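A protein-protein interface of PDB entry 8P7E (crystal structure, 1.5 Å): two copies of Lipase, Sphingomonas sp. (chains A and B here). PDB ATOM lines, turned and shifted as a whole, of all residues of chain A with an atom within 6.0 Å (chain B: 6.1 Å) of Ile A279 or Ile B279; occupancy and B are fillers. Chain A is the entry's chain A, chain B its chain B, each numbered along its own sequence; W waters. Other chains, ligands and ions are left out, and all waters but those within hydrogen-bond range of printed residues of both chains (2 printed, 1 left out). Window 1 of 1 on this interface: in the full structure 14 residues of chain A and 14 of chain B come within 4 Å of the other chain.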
ATOM      1  N   GLY A 271     -12.579  -3.936 -11.338  1.00  0.00           N
ATOM      2  CA  GLY A 271     -12.254  -2.695 -10.638  1.00  0.00           C
ATOM      3  C   GLY A 271     -11.805  -2.915  -9.204  1.00  0.00           C
ATOM      4  O   GLY A 271     -10.826  -2.332  -8.743  1.00  0.00           O
ATOM      5  N   ARG A 272     -12.517  -3.794  -8.478  1.00  0.00           N
ATOM      6  CA  ARG A 272     -12.070  -4.200  -7.169  1.00  0.00           C
ATOM      7  C   ARG A 272     -10.656  -4.754  -7.240  1.00  0.00           C
ATOM      8  O   ARG A 272      -9.805  -4.475  -6.414  1.00  0.00           O
ATOM      9  CB  ARG A 272     -13.001  -5.271  -6.604  1.00  0.00           C
ATOM     10  CG  ARG A 272     -14.387  -4.806  -6.186  1.00  0.00           C
ATOM     11  CD  ARG A 272     -15.255  -5.991  -5.795  1.00  0.00           C
ATOM     12  NE  ARG A 272     -16.579  -5.626  -5.268  1.00  0.00           N
ATOM     13  CZ  ARG A 272     -17.446  -6.535  -4.864  1.00  0.00           C
ATOM     14  NH1 ARG A 272     -17.144  -7.811  -4.924  1.00  0.00           N
ATOM     15  NH2 ARG A 272     -18.612  -6.152  -4.420  1.00  0.00           N
ATOM     16  N   ALA A 273     -10.411  -5.619  -8.233  1.00  0.00           N
ATOM     17  CA  ALA A 273      -9.097  -6.237  -8.365  1.00  0.00           C
ATOM     18  C   ALA A 273      -8.001  -5.226  -8.630  1.00  0.00           C
ATOM     19  O   ALA A 273      -6.913  -5.368  -8.075  1.00  0.00           O
ATOM     20  CB  ALA A 273      -9.150  -7.293  -9.426  1.00  0.00           C
ATOM     21  N   TYR A 274      -8.283  -4.215  -9.434  1.00  0.00           N
ATOM     22  CA  TYR A 274      -7.250  -3.233  -9.693  1.00  0.00           C
ATOM     23  C   TYR A 274      -6.979  -2.408  -8.423  1.00  0.00           C
ATOM     24  O   TYR A 274      -5.805  -2.070  -8.143  1.00  0.00           O
ATOM     25  CB  TYR A 274      -7.596  -2.356 -10.899  1.00  0.00           C
ATOM     26  CG  TYR A 274      -6.402  -1.607 -11.428  1.00  0.00           C
ATOM     27  CD1 TYR A 274      -5.459  -2.283 -12.173  1.00  0.00           C
ATOM     28  CD2 TYR A 274      -6.140  -0.304 -11.065  1.00  0.00           C
ATOM     29  CE1 TYR A 274      -4.292  -1.679 -12.581  1.00  0.00           C
ATOM     30  CE2 TYR A 274      -4.955   0.312 -11.416  1.00  0.00           C
ATOM     31  CZ  TYR A 274      -4.020  -0.382 -12.171  1.00  0.00           C
ATOM     32  OH  TYR A 274      -2.837   0.239 -12.499  1.00  0.00           O
ATOM     33  N   ALA A 275      -8.045  -2.040  -7.693  1.00  0.00           N
ATOM     34  CA  ALA A 275      -7.835  -1.281  -6.467  1.00  0.00           C
ATOM     35  C   ALA A 275      -7.018  -2.094  -5.464  1.00  0.00           C
ATOM     36  O   ALA A 275      -6.114  -1.557  -4.811  1.00  0.00           O
ATOM     37  CB  ALA A 275      -9.168  -0.881  -5.898  1.00  0.00           C
ATOM     38  N   ALA A 276      -7.297  -3.389  -5.371  1.00  0.00           N
ATOM     39  CA  ALA A 276      -6.547  -4.282  -4.487  1.00  0.00           C
ATOM     40  C   ALA A 276      -5.090  -4.334  -4.921  1.00  0.00           C
ATOM     41  O   ALA A 276      -4.162  -4.312  -4.103  1.00  0.00           O
ATOM     42  CB  ALA A 276      -7.173  -5.650  -4.472  1.00  0.00           C
ATOM     43  N   LYS A 277      -4.829  -4.370  -6.230  1.00  0.00           N
ATOM     44  CA  LYS A 277      -3.470  -4.388  -6.770  1.00  0.00           C
ATOM     45  C   LYS A 277      -2.702  -3.107  -6.421  1.00  0.00           C
ATOM     46  O   LYS A 277      -1.509  -3.110  -6.073  1.00  0.00           O
ATOM     47  CB  LYS A 277      -3.543  -4.565  -8.285  1.00  0.00           C
ATOM     48  CG  LYS A 277      -2.237  -4.533  -9.051  1.00  0.00           C
ATOM     49  CD  LYS A 277      -2.501  -4.517 -10.552  1.00  0.00           C
ATOM     50  CE  LYS A 277      -1.253  -4.398 -11.386  1.00  0.00           C
ATOM     51  NZ  LYS A 277      -0.434  -5.604 -11.273  1.00  0.00           N
ATOM     52  N   LEU A 278      -3.375  -1.971  -6.511  1.00  0.00           N
ATOM     53  CA  LEU A 278      -2.759  -0.708  -6.135  1.00  0.00           C
ATOM     54  C   LEU A 278      -2.292  -0.778  -4.677  1.00  0.00           C
ATOM     55  O   LEU A 278      -1.197  -0.312  -4.370  1.00  0.00           O
ATOM     56  CB  LEU A 278      -3.745   0.435  -6.345  1.00  0.00           C
ATOM     57  CG  LEU A 278      -3.993   0.823  -7.796  1.00  0.00           C
ATOM     58  CD1 LEU A 278      -5.214   1.689  -7.924  1.00  0.00           C
ATOM     59  CD2 LEU A 278      -2.801   1.546  -8.376  1.00  0.00           C
ATOM     60  N   ILE A 279      -3.171  -1.220  -3.792  1.00  0.00           N
ATOM     61  CA  ILE A 279      -2.845  -1.267  -2.364  1.00  0.00           C
ATOM     62  C   ILE A 279      -1.669  -2.226  -2.141  1.00  0.00           C
ATOM     63  O   ILE A 279      -0.748  -1.886  -1.402  1.00  0.00           O
ATOM     64  CB  ILE A 279      -4.053  -1.672  -1.552  1.00  0.00           C
ATOM     65  CG1 ILE A 279      -5.079  -0.551  -1.597  1.00  0.00           C
ATOM     66  CG2 ILE A 279      -3.635  -2.066  -0.133  1.00  0.00           C
ATOM     67  CD1 ILE A 279      -6.337  -0.954  -1.045  1.00  0.00           C
ATOM     68  N   GLU A 280      -1.658  -3.365  -2.825  1.00  0.00           N
ATOM     69  CA  GLU A 280      -0.571  -4.322  -2.659  1.00  0.00           C
ATOM     70  C   GLU A 280       0.746  -3.754  -3.156  1.00  0.00           C
ATOM     71  O   GLU A 280       1.775  -4.192  -2.652  1.00  0.00           O
ATOM     72  CB  GLU A 280      -0.857  -5.629  -3.394  1.00  0.00           C
ATOM     73  CG  GLU A 280      -1.980  -6.428  -2.787  1.00  0.00           C
ATOM     74  CD  GLU A 280      -2.581  -7.452  -3.735  1.00  0.00           C
ATOM     75  OE1 GLU A 280      -1.940  -7.738  -4.759  1.00  0.00           O
ATOM     76  OE2 GLU A 280      -3.745  -7.864  -3.516  1.00  0.00           O
ATOM     77  N   ALA A 281       0.716  -2.741  -4.042  1.00  0.00           N
ATOM     78  CA  ALA A 281       1.902  -2.038  -4.492  1.00  0.00           C
ATOM     79  C   ALA A 281       2.214  -0.794  -3.669  1.00  0.00           C
ATOM     80  O   ALA A 281       3.117  -0.040  -4.051  1.00  0.00           O
ATOM     81  CB  ALA A 281       1.702  -1.651  -5.928  1.00  0.00           C
ATOM     82  N   GLY A 282       1.481  -0.518  -2.603  1.00  0.00           N
ATOM     83  CA  GLY A 282       1.763   0.608  -1.757  1.00  0.00           C
ATOM     84  C   GLY A 282       1.185   1.941  -2.231  1.00  0.00           C
ATOM     85  O   GLY A 282       1.558   3.011  -1.729  1.00  0.00           O
ATOM     86  N   VAL A 283       0.296   1.901  -3.197  1.00  0.00           N
ATOM     87  CA  VAL A 283      -0.299   3.141  -3.678  1.00  0.00           C
ATOM     88  C   VAL A 283      -1.452   3.533  -2.783  1.00  0.00           C
ATOM     89  O   VAL A 283      -2.383   2.730  -2.571  1.00  0.00           O
ATOM     90  CB  VAL A 283      -0.794   2.977  -5.126  1.00  0.00           C
ATOM     91  CG1 VAL A 283      -1.492   4.235  -5.639  1.00  0.00           C
ATOM     92  CG2 VAL A 283       0.297   2.526  -6.064  1.00  0.00           C
ATOM     93  N   PRO A 284      -1.516   4.760  -2.266  1.00  0.00           N
ATOM     94  CA  PRO A 284      -2.659   5.170  -1.465  1.00  0.00           C
ATOM     95  C   PRO A 284      -3.933   5.201  -2.284  1.00  0.00           C
ATOM     96  O   PRO A 284      -3.921   5.694  -3.444  1.00  0.00           O
ATOM     97  CB  PRO A 284      -2.330   6.573  -0.998  1.00  0.00           C
ATOM     98  CG  PRO A 284      -0.929   6.857  -1.398  1.00  0.00           C
ATOM     99  CD  PRO A 284      -0.479   5.791  -2.355  1.00  0.00           C
ATOM    100  N   THR A 285      -4.923   4.491  -1.841  1.00  0.00           N
ATOM    101  CA  THR A 285      -6.065   4.104  -2.656  1.00  0.00           C
ATOM    102  C   THR A 285      -7.331   4.289  -1.851  1.00  0.00           C
ATOM    103  O   THR A 285      -7.425   3.762  -0.743  1.00  0.00           O
ATOM    104  CB  THR A 285      -6.003   2.640  -3.129  1.00  0.00           C
ATOM    105  OG1 THR A 285      -4.819   2.559  -3.917  1.00  0.00           O
ATOM    106  CG2 THR A 285      -7.136   2.183  -4.016  1.00  0.00           C
ATOM    107  N   TYR A 287     -11.267   3.300  -2.297  1.00  0.00           N
ATOM    108  CA  TYR A 287     -12.180   2.458  -3.041  1.00  0.00           C
ATOM    109  C   TYR A 287     -13.605   2.768  -2.597  1.00  0.00           C
ATOM    110  O   TYR A 287     -13.953   2.678  -1.429  1.00  0.00           O
ATOM    111  CB  TYR A 287     -11.877   0.976  -2.818  1.00  0.00           C
ATOM    112  CG  TYR A 287     -12.879   0.099  -3.482  1.00  0.00           C
ATOM    113  CD1 TYR A 287     -12.823  -0.001  -4.858  1.00  0.00           C
ATOM    114  CD2 TYR A 287     -13.906  -0.536  -2.799  1.00  0.00           C
ATOM    115  CE1 TYR A 287     -13.780  -0.707  -5.539  1.00  0.00           C
ATOM    116  CE2 TYR A 287     -14.883  -1.265  -3.474  1.00  0.00           C
ATOM    117  CZ  TYR A 287     -14.807  -1.322  -4.854  1.00  0.00           C
ATOM    118  OH  TYR A 287     -15.774  -2.008  -5.597  1.00  0.00           O
ATOM    119  N   GLU A 289     -17.802   2.009  -3.777  1.00  0.00           N
ATOM    120  CA  GLU A 289     -18.656   1.127  -4.576  1.00  0.00           C
ATOM    121  C   GLU A 289     -20.055   1.713  -4.469  1.00  0.00           C
ATOM    122  O   GLU A 289     -20.623   1.779  -3.370  1.00  0.00           O
ATOM    123  CB  GLU A 289     -18.579  -0.297  -4.060  1.00  0.00           C
ATOM    124  CG  GLU A 289     -19.344  -1.323  -4.884  1.00  0.00           C
ATOM    125  CD  GLU A 289     -18.952  -2.765  -4.615  1.00  0.00           C
ATOM    126  OE1 GLU A 289     -17.723  -3.146  -4.575  1.00  0.00           O
ATOM    127  OE2 GLU A 289     -19.910  -3.588  -4.527  1.00  0.00           O
ATOM    128  N   GLY B 271      -1.148  -5.571   6.482  1.00  0.00           N
ATOM    129  CA  GLY B 271      -2.122  -4.499   6.439  1.00  0.00           C
ATOM    130  C   GLY B 271      -2.609  -4.210   5.032  1.00  0.00           C
ATOM    131  O   GLY B 271      -3.825  -4.066   4.806  1.00  0.00           O
ATOM    132  N   ARG B 272      -1.660  -4.129   4.089  1.00  0.00           N
ATOM    133  CA  ARG B 272      -2.010  -4.019   2.685  1.00  0.00           C
ATOM    134  C   ARG B 272      -2.930  -5.155   2.279  1.00  0.00           C
ATOM    135  O   ARG B 272      -3.952  -4.977   1.601  1.00  0.00           O
ATOM    136  CB  ARG B 272      -0.758  -4.055   1.817  1.00  0.00           C
ATOM    137  CG  ARG B 272       0.106  -2.807   1.858  1.00  0.00           C
ATOM    138  CD  ARG B 272       1.337  -2.997   1.014  1.00  0.00           C
ATOM    139  NE  ARG B 272       2.248  -1.867   0.969  1.00  0.00           N
ATOM    140  CZ  ARG B 272       3.375  -1.868   0.278  1.00  0.00           C
ATOM    141  NH1 ARG B 272       3.761  -2.962  -0.325  1.00  0.00           N
ATOM    142  NH2 ARG B 272       4.162  -0.819   0.290  1.00  0.00           N
ATOM    143  N   ALA B 273      -2.573  -6.386   2.678  1.00  0.00           N
ATOM    144  CA  ALA B 273      -3.340  -7.553   2.289  1.00  0.00           C
ATOM    145  C   ALA B 273      -4.747  -7.499   2.853  1.00  0.00           C
ATOM    146  O   ALA B 273      -5.685  -7.894   2.151  1.00  0.00           O
ATOM    147  CB  ALA B 273      -2.616  -8.782   2.724  1.00  0.00           C
ATOM    148  N   TYR B 274      -4.894  -7.056   4.088  1.00  0.00           N
ATOM    149  CA  TYR B 274      -6.231  -6.976   4.659  1.00  0.00           C
ATOM    150  C   TYR B 274      -7.091  -5.908   3.935  1.00  0.00           C
ATOM    151  O   TYR B 274      -8.276  -6.124   3.677  1.00  0.00           O
ATOM    152  CB  TYR B 274      -6.230  -6.741   6.180  1.00  0.00           C
ATOM    153  CG  TYR B 274      -7.560  -7.091   6.775  1.00  0.00           C
ATOM    154  CD1 TYR B 274      -7.942  -8.408   6.961  1.00  0.00           C
ATOM    155  CD2 TYR B 274      -8.494  -6.122   7.120  1.00  0.00           C
ATOM    156  CE1 TYR B 274      -9.186  -8.766   7.434  1.00  0.00           C
ATOM    157  CE2 TYR B 274      -9.757  -6.450   7.574  1.00  0.00           C
ATOM    158  CZ  TYR B 274     -10.114  -7.784   7.705  1.00  0.00           C
ATOM    159  OH  TYR B 274     -11.362  -8.116   8.143  1.00  0.00           O
ATOM    160  N   ALA B 275      -6.493  -4.754   3.622  1.00  0.00           N
ATOM    161  CA  ALA B 275      -7.237  -3.739   2.905  1.00  0.00           C
ATOM    162  C   ALA B 275      -7.658  -4.258   1.536  1.00  0.00           C
ATOM    163  O   ALA B 275      -8.776  -4.008   1.079  1.00  0.00           O
ATOM    164  CB  ALA B 275      -6.394  -2.509   2.796  1.00  0.00           C
ATOM    165  N   ALA B 276      -6.768  -5.013   0.850  1.00  0.00           N
ATOM    166  CA  ALA B 276      -7.100  -5.603  -0.445  1.00  0.00           C
ATOM    167  C   ALA B 276      -8.266  -6.570  -0.299  1.00  0.00           C
ATOM    168  O   ALA B 276      -9.160  -6.583  -1.135  1.00  0.00           O
ATOM    169  CB  ALA B 276      -5.883  -6.245  -1.054  1.00  0.00           C
ATOM    170  N   LYS B 277      -8.255  -7.364   0.778  1.00  0.00           N
ATOM    171  CA  LYS B 277      -9.323  -8.324   1.030  1.00  0.00           C
ATOM    172  C   LYS B 277     -10.664  -7.624   1.228  1.00  0.00           C
ATOM    173  O   LYS B 277     -11.714  -8.079   0.756  1.00  0.00           O
ATOM    174  CB  LYS B 277      -8.905  -9.186   2.227  1.00  0.00           C
ATOM    175  CG  LYS B 277      -9.939 -10.121   2.756  1.00  0.00           C
ATOM    176  CD  LYS B 277      -9.436 -10.801   4.034  1.00  0.00           C
ATOM    177  CE  LYS B 277     -10.477 -11.711   4.641  1.00  0.00           C
ATOM    178  NZ  LYS B 277     -10.645 -12.936   3.847  1.00  0.00           N
ATOM    179  N   LEU B 278     -10.670  -6.509   1.944  1.00  0.00           N
ATOM    180  CA  LEU B 278     -11.875  -5.742   2.162  1.00  0.00           C
ATOM    181  C   LEU B 278     -12.455  -5.296   0.822  1.00  0.00           C
ATOM    182  O   LEU B 278     -13.670  -5.423   0.636  1.00  0.00           O
ATOM    183  CB  LEU B 278     -11.568  -4.550   3.058  1.00  0.00           C
ATOM    184  CG  LEU B 278     -11.340  -4.843   4.545  1.00  0.00           C
ATOM    185  CD1 LEU B 278     -10.744  -3.646   5.202  1.00  0.00           C
ATOM    186  CD2 LEU B 278     -12.637  -5.189   5.217  1.00  0.00           C
ATOM    187  N   ILE B 279     -11.611  -4.757  -0.046  1.00  0.00           N
ATOM    188  CA  ILE B 279     -12.099  -4.281  -1.332  1.00  0.00           C
ATOM    189  C   ILE B 279     -12.647  -5.460  -2.150  1.00  0.00           C
ATOM    190  O   ILE B 279     -13.688  -5.308  -2.788  1.00  0.00           O
ATOM    191  CB  ILE B 279     -10.971  -3.556  -2.053  1.00  0.00           C
ATOM    192  CG1 ILE B 279     -10.673  -2.244  -1.325  1.00  0.00           C
ATOM    193  CG2 ILE B 279     -11.309  -3.339  -3.502  1.00  0.00           C
ATOM    194  CD1 ILE B 279      -9.476  -1.572  -1.802  1.00  0.00           C
ATOM    195  N   GLU B 280     -11.975  -6.596  -2.155  1.00  0.00           N
ATOM    196  CA  GLU B 280     -12.449  -7.745  -2.912  1.00  0.00           C
ATOM    197  C   GLU B 280     -13.760  -8.269  -2.372  1.00  0.00           C
ATOM    198  O   GLU B 280     -14.499  -8.876  -3.140  1.00  0.00           O
ATOM    199  CB  GLU B 280     -11.400  -8.842  -2.933  1.00  0.00           C
ATOM    200  CG  GLU B 280     -10.180  -8.482  -3.753  1.00  0.00           C
ATOM    201  CD  GLU B 280      -8.984  -9.388  -3.514  1.00  0.00           C
ATOM    202  OE1 GLU B 280      -9.129 -10.387  -2.731  1.00  0.00           O
ATOM    203  OE2 GLU B 280      -7.919  -9.101  -4.081  1.00  0.00           O
ATOM    204  N   ALA B 281     -14.130  -7.919  -1.127  1.00  0.00           N
ATOM    205  CA  ALA B 281     -15.421  -8.236  -0.536  1.00  0.00           C
ATOM    206  C   ALA B 281     -16.444  -7.115  -0.703  1.00  0.00           C
ATOM    207  O   ALA B 281     -17.539  -7.216  -0.141  1.00  0.00           O
ATOM    208  CB  ALA B 281     -15.243  -8.589   0.911  1.00  0.00           C
ATOM    209  N   GLY B 282     -16.098  -6.031  -1.404  1.00  0.00           N
ATOM    210  CA  GLY B 282     -17.013  -4.923  -1.591  1.00  0.00           C
ATOM    211  C   GLY B 282     -17.170  -3.967  -0.417  1.00  0.00           C
ATOM    212  O   GLY B 282     -18.133  -3.185  -0.367  1.00  0.00           O
ATOM    213  N   VAL B 283     -16.236  -4.016   0.531  1.00  0.00           N
ATOM    214  CA  VAL B 283     -16.287  -3.087   1.634  1.00  0.00           C
ATOM    215  C   VAL B 283     -15.668  -1.755   1.204  1.00  0.00           C
ATOM    216  O   VAL B 283     -14.544  -1.743   0.717  1.00  0.00           O
ATOM    217  CB  VAL B 283     -15.544  -3.653   2.859  1.00  0.00           C
ATOM    218  CG1 VAL B 283     -15.565  -2.647   4.015  1.00  0.00           C
ATOM    219  CG2 VAL B 283     -16.100  -4.997   3.280  1.00  0.00           C
ATOM    220  N   PRO B 284     -16.323  -0.623   1.377  1.00  0.00           N
ATOM    221  CA  PRO B 284     -15.707   0.650   1.050  1.00  0.00           C
ATOM    222  C   PRO B 284     -14.501   0.872   1.941  1.00  0.00           C
ATOM    223  O   PRO B 284     -14.581   0.741   3.184  1.00  0.00           O
ATOM    224  CB  PRO B 284     -16.742   1.725   1.425  1.00  0.00           C
ATOM    225  CG  PRO B 284     -18.029   0.989   1.702  1.00  0.00           C
ATOM    226  CD  PRO B 284     -17.707  -0.481   1.854  1.00  0.00           C
ATOM    227  N   THR B 285     -13.366   1.141   1.341  1.00  0.00           N
ATOM    228  CA  THR B 285     -12.079   1.024   2.018  1.00  0.00           C
ATOM    229  C   THR B 285     -11.202   2.194   1.592  1.00  0.00           C
ATOM    230  O   THR B 285     -11.070   2.478   0.397  1.00  0.00           O
ATOM    231  CB  THR B 285     -11.328  -0.275   1.679  1.00  0.00           C
ATOM    232  OG1 THR B 285     -12.179  -1.357   2.079  1.00  0.00           O
ATOM    233  CG2 THR B 285     -10.015  -0.463   2.393  1.00  0.00           C
ATOM    234  N   TYR B 287      -7.319   3.278   2.021  1.00  0.00           N
ATOM    235  CA  TYR B 287      -6.001   2.787   2.405  1.00  0.00           C
ATOM    236  C   TYR B 287      -5.013   3.931   2.353  1.00  0.00           C
ATOM    237  O   TYR B 287      -4.862   4.604   1.331  1.00  0.00           O
ATOM    238  CB  TYR B 287      -5.553   1.668   1.466  1.00  0.00           C
ATOM    239  CG  TYR B 287      -4.159   1.202   1.730  1.00  0.00           C
ATOM    240  CD1 TYR B 287      -3.921   0.468   2.868  1.00  0.00           C
ATOM    241  CD2 TYR B 287      -3.089   1.618   0.979  1.00  0.00           C
ATOM    242  CE1 TYR B 287      -2.646   0.116   3.240  1.00  0.00           C
ATOM    243  CE2 TYR B 287      -1.783   1.237   1.326  1.00  0.00           C
ATOM    244  CZ  TYR B 287      -1.573   0.518   2.481  1.00  0.00           C
ATOM    245  OH  TYR B 287      -0.339   0.169   2.930  1.00  0.00           O
ATOM    246  N   GLU B 289      -0.864   4.910   3.513  1.00  0.00           N
ATOM    247  CA  GLU B 289       0.432   4.351   3.904  1.00  0.00           C
ATOM    248  C   GLU B 289       1.311   5.537   4.297  1.00  0.00           C
ATOM    249  O   GLU B 289       1.591   6.431   3.474  1.00  0.00           O
ATOM    250  CB  GLU B 289       1.001   3.530   2.753  1.00  0.00           C
ATOM    251  CG  GLU B 289       2.298   2.805   3.090  1.00  0.00           C
ATOM    252  CD  GLU B 289       2.665   1.669   2.140  1.00  0.00           C
ATOM    253  OE1 GLU B 289       1.794   0.802   1.757  1.00  0.00           O
ATOM    254  OE2 GLU B 289       3.863   1.618   1.806  1.00  0.00           O
HETATM  255  O   HOH W   1       2.684  -5.787  -0.511  1.00  0.00           O
HETATM  256  O   HOH W   2     -14.656  -9.427  -5.885  1.00  0.00           O
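O of Glu B280 sits at hydrogen-bond distance from NH1 of Arg A272 (3.4 Å). NH1 of Arg B272 sits at hydrogen-bond distance from O of Glu A280 (3.3 Å). O of Thr A285 lies within hydrogen-bond range of N of Tyr B287, 2.8 Å away. O of Thr B285 sits at hydrogen-bond distance from N of Tyr A287, at 2.8 Å.
Ala B276 touches Ala A276 (CB to CB, 3.7 Å). Ala A276 touches Glu B280 (CB to OE2, 3.6 Å). Arg B272 touches Ile A279 (CD to O, 3.4 Å). Ile A279 touches Ile B279. CD1 of Ile A279 touches CB of Tyr B287 (3.7 Å). CB of Ala B276 touches OE2 of Glu A280, at 3.6 Å. Gly A282 touches Arg B272 (CA to NH2, 3.5 Å). Tyr B287 touches Pro A284. Val B283 touches Tyr A287. O of Tyr A287 touches CA of Pro B284, at 3.7 Å.
Of chain B, only Arg B272, Ile B279 and Tyr B287 come within 4 Å of Ile A279. Of the printed residues of chain A, Ile B279 touches Arg A272, Ile A279 and Tyr A287. Of the printed residues of chain B, Pro A284 touches Tyr B287. Of the printed residues of chain A, Glu B289 touches Gly A282 (3.5 Å). The nearest residue of chain A that does not touch Ile B279 is Ala A275 (4.05 Å).
Arg A272 touches Ile B279, and with the chains exchanged Ile A279 touches Arg B272. Ala A276 touches its own counterpart, Ala B276. Ala A276 touches Glu B280, and with the chains exchanged Glu A280 touches Ala B276. Gly A282 touches Glu B289, and with the chains exchanged Glu A289 touches Gly B282. Positions printed for both chains: 271, 272, 273, 274, 275, 276, 277, 278, 279, 280, 281, 282, 283, 284, 285, 287 and 289. Of the 20 pairs that touch across the chains among the printed residues, 20 have their exchanged pair printed and touching as well.
Of the 17 printed residues of chain A, 10 touch a printed residue of chain B. Printed residues of chain A that touch a printed residue of chain B: Arg A272, Ala A276, Ile A279, Glu A280, Gly A282, Val A283, Pro A284, Thr A285, Tyr A287 and Glu A289. Of the 17 printed residues of chain B, 10 touch a printed residue of chain A. Printed residues of chain B that touch a printed residue of chain A: Arg B272, Ala B276, Ile B279, Glu B280, Gly B282, Val B283, Pro B284, Thr B285, Tyr B287 and Glu B289. Hydrophobic or aromatic side chains of chain B that line the printed part of chain A: Ala B276, Ile B279 and Tyr B287. Among the printed residues, 20 pairs touch across the chains.
The guanidinium group of Arg A272 lies within salt-bridge range of the side-chain carboxylate of Glu A289 (2.8 Å). The backbone carbonyl oxygen of Leu A278 sits at hydrogen-bond distance from the backbone NH of Val A283 (2.9 Å). The side-chain hydroxyl of Tyr A287 is in hydrogen-bond range of the side-chain carboxylate of Glu A289, 2.5 Å away. The guanidinium group of Arg B272 lies within salt-bridge range of the side-chain carboxylate of Glu B289 (2.8 Å). The backbone carbonyl oxygen of Leu B278 is in hydrogen-bond range of the backbone NH of Val B283 (2.9 Å). The side-chain carboxylate (OE1) of Glu B289 lies within hydrogen-bond range of the side-chain hydroxyl (OH) of Tyr B287, at 2.5 Å.
Water W2 bridges the backbone carbonyl oxygen of Glu B280 (2.8 Å) and the guanidinium group of Arg A272 (3.1 Å). Water W1 lies within hydrogen-bond range of the backbone carbonyl oxygen of Glu A280 (2.8 Å) and the guanidinium group of Arg B272 (3.0 Å).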
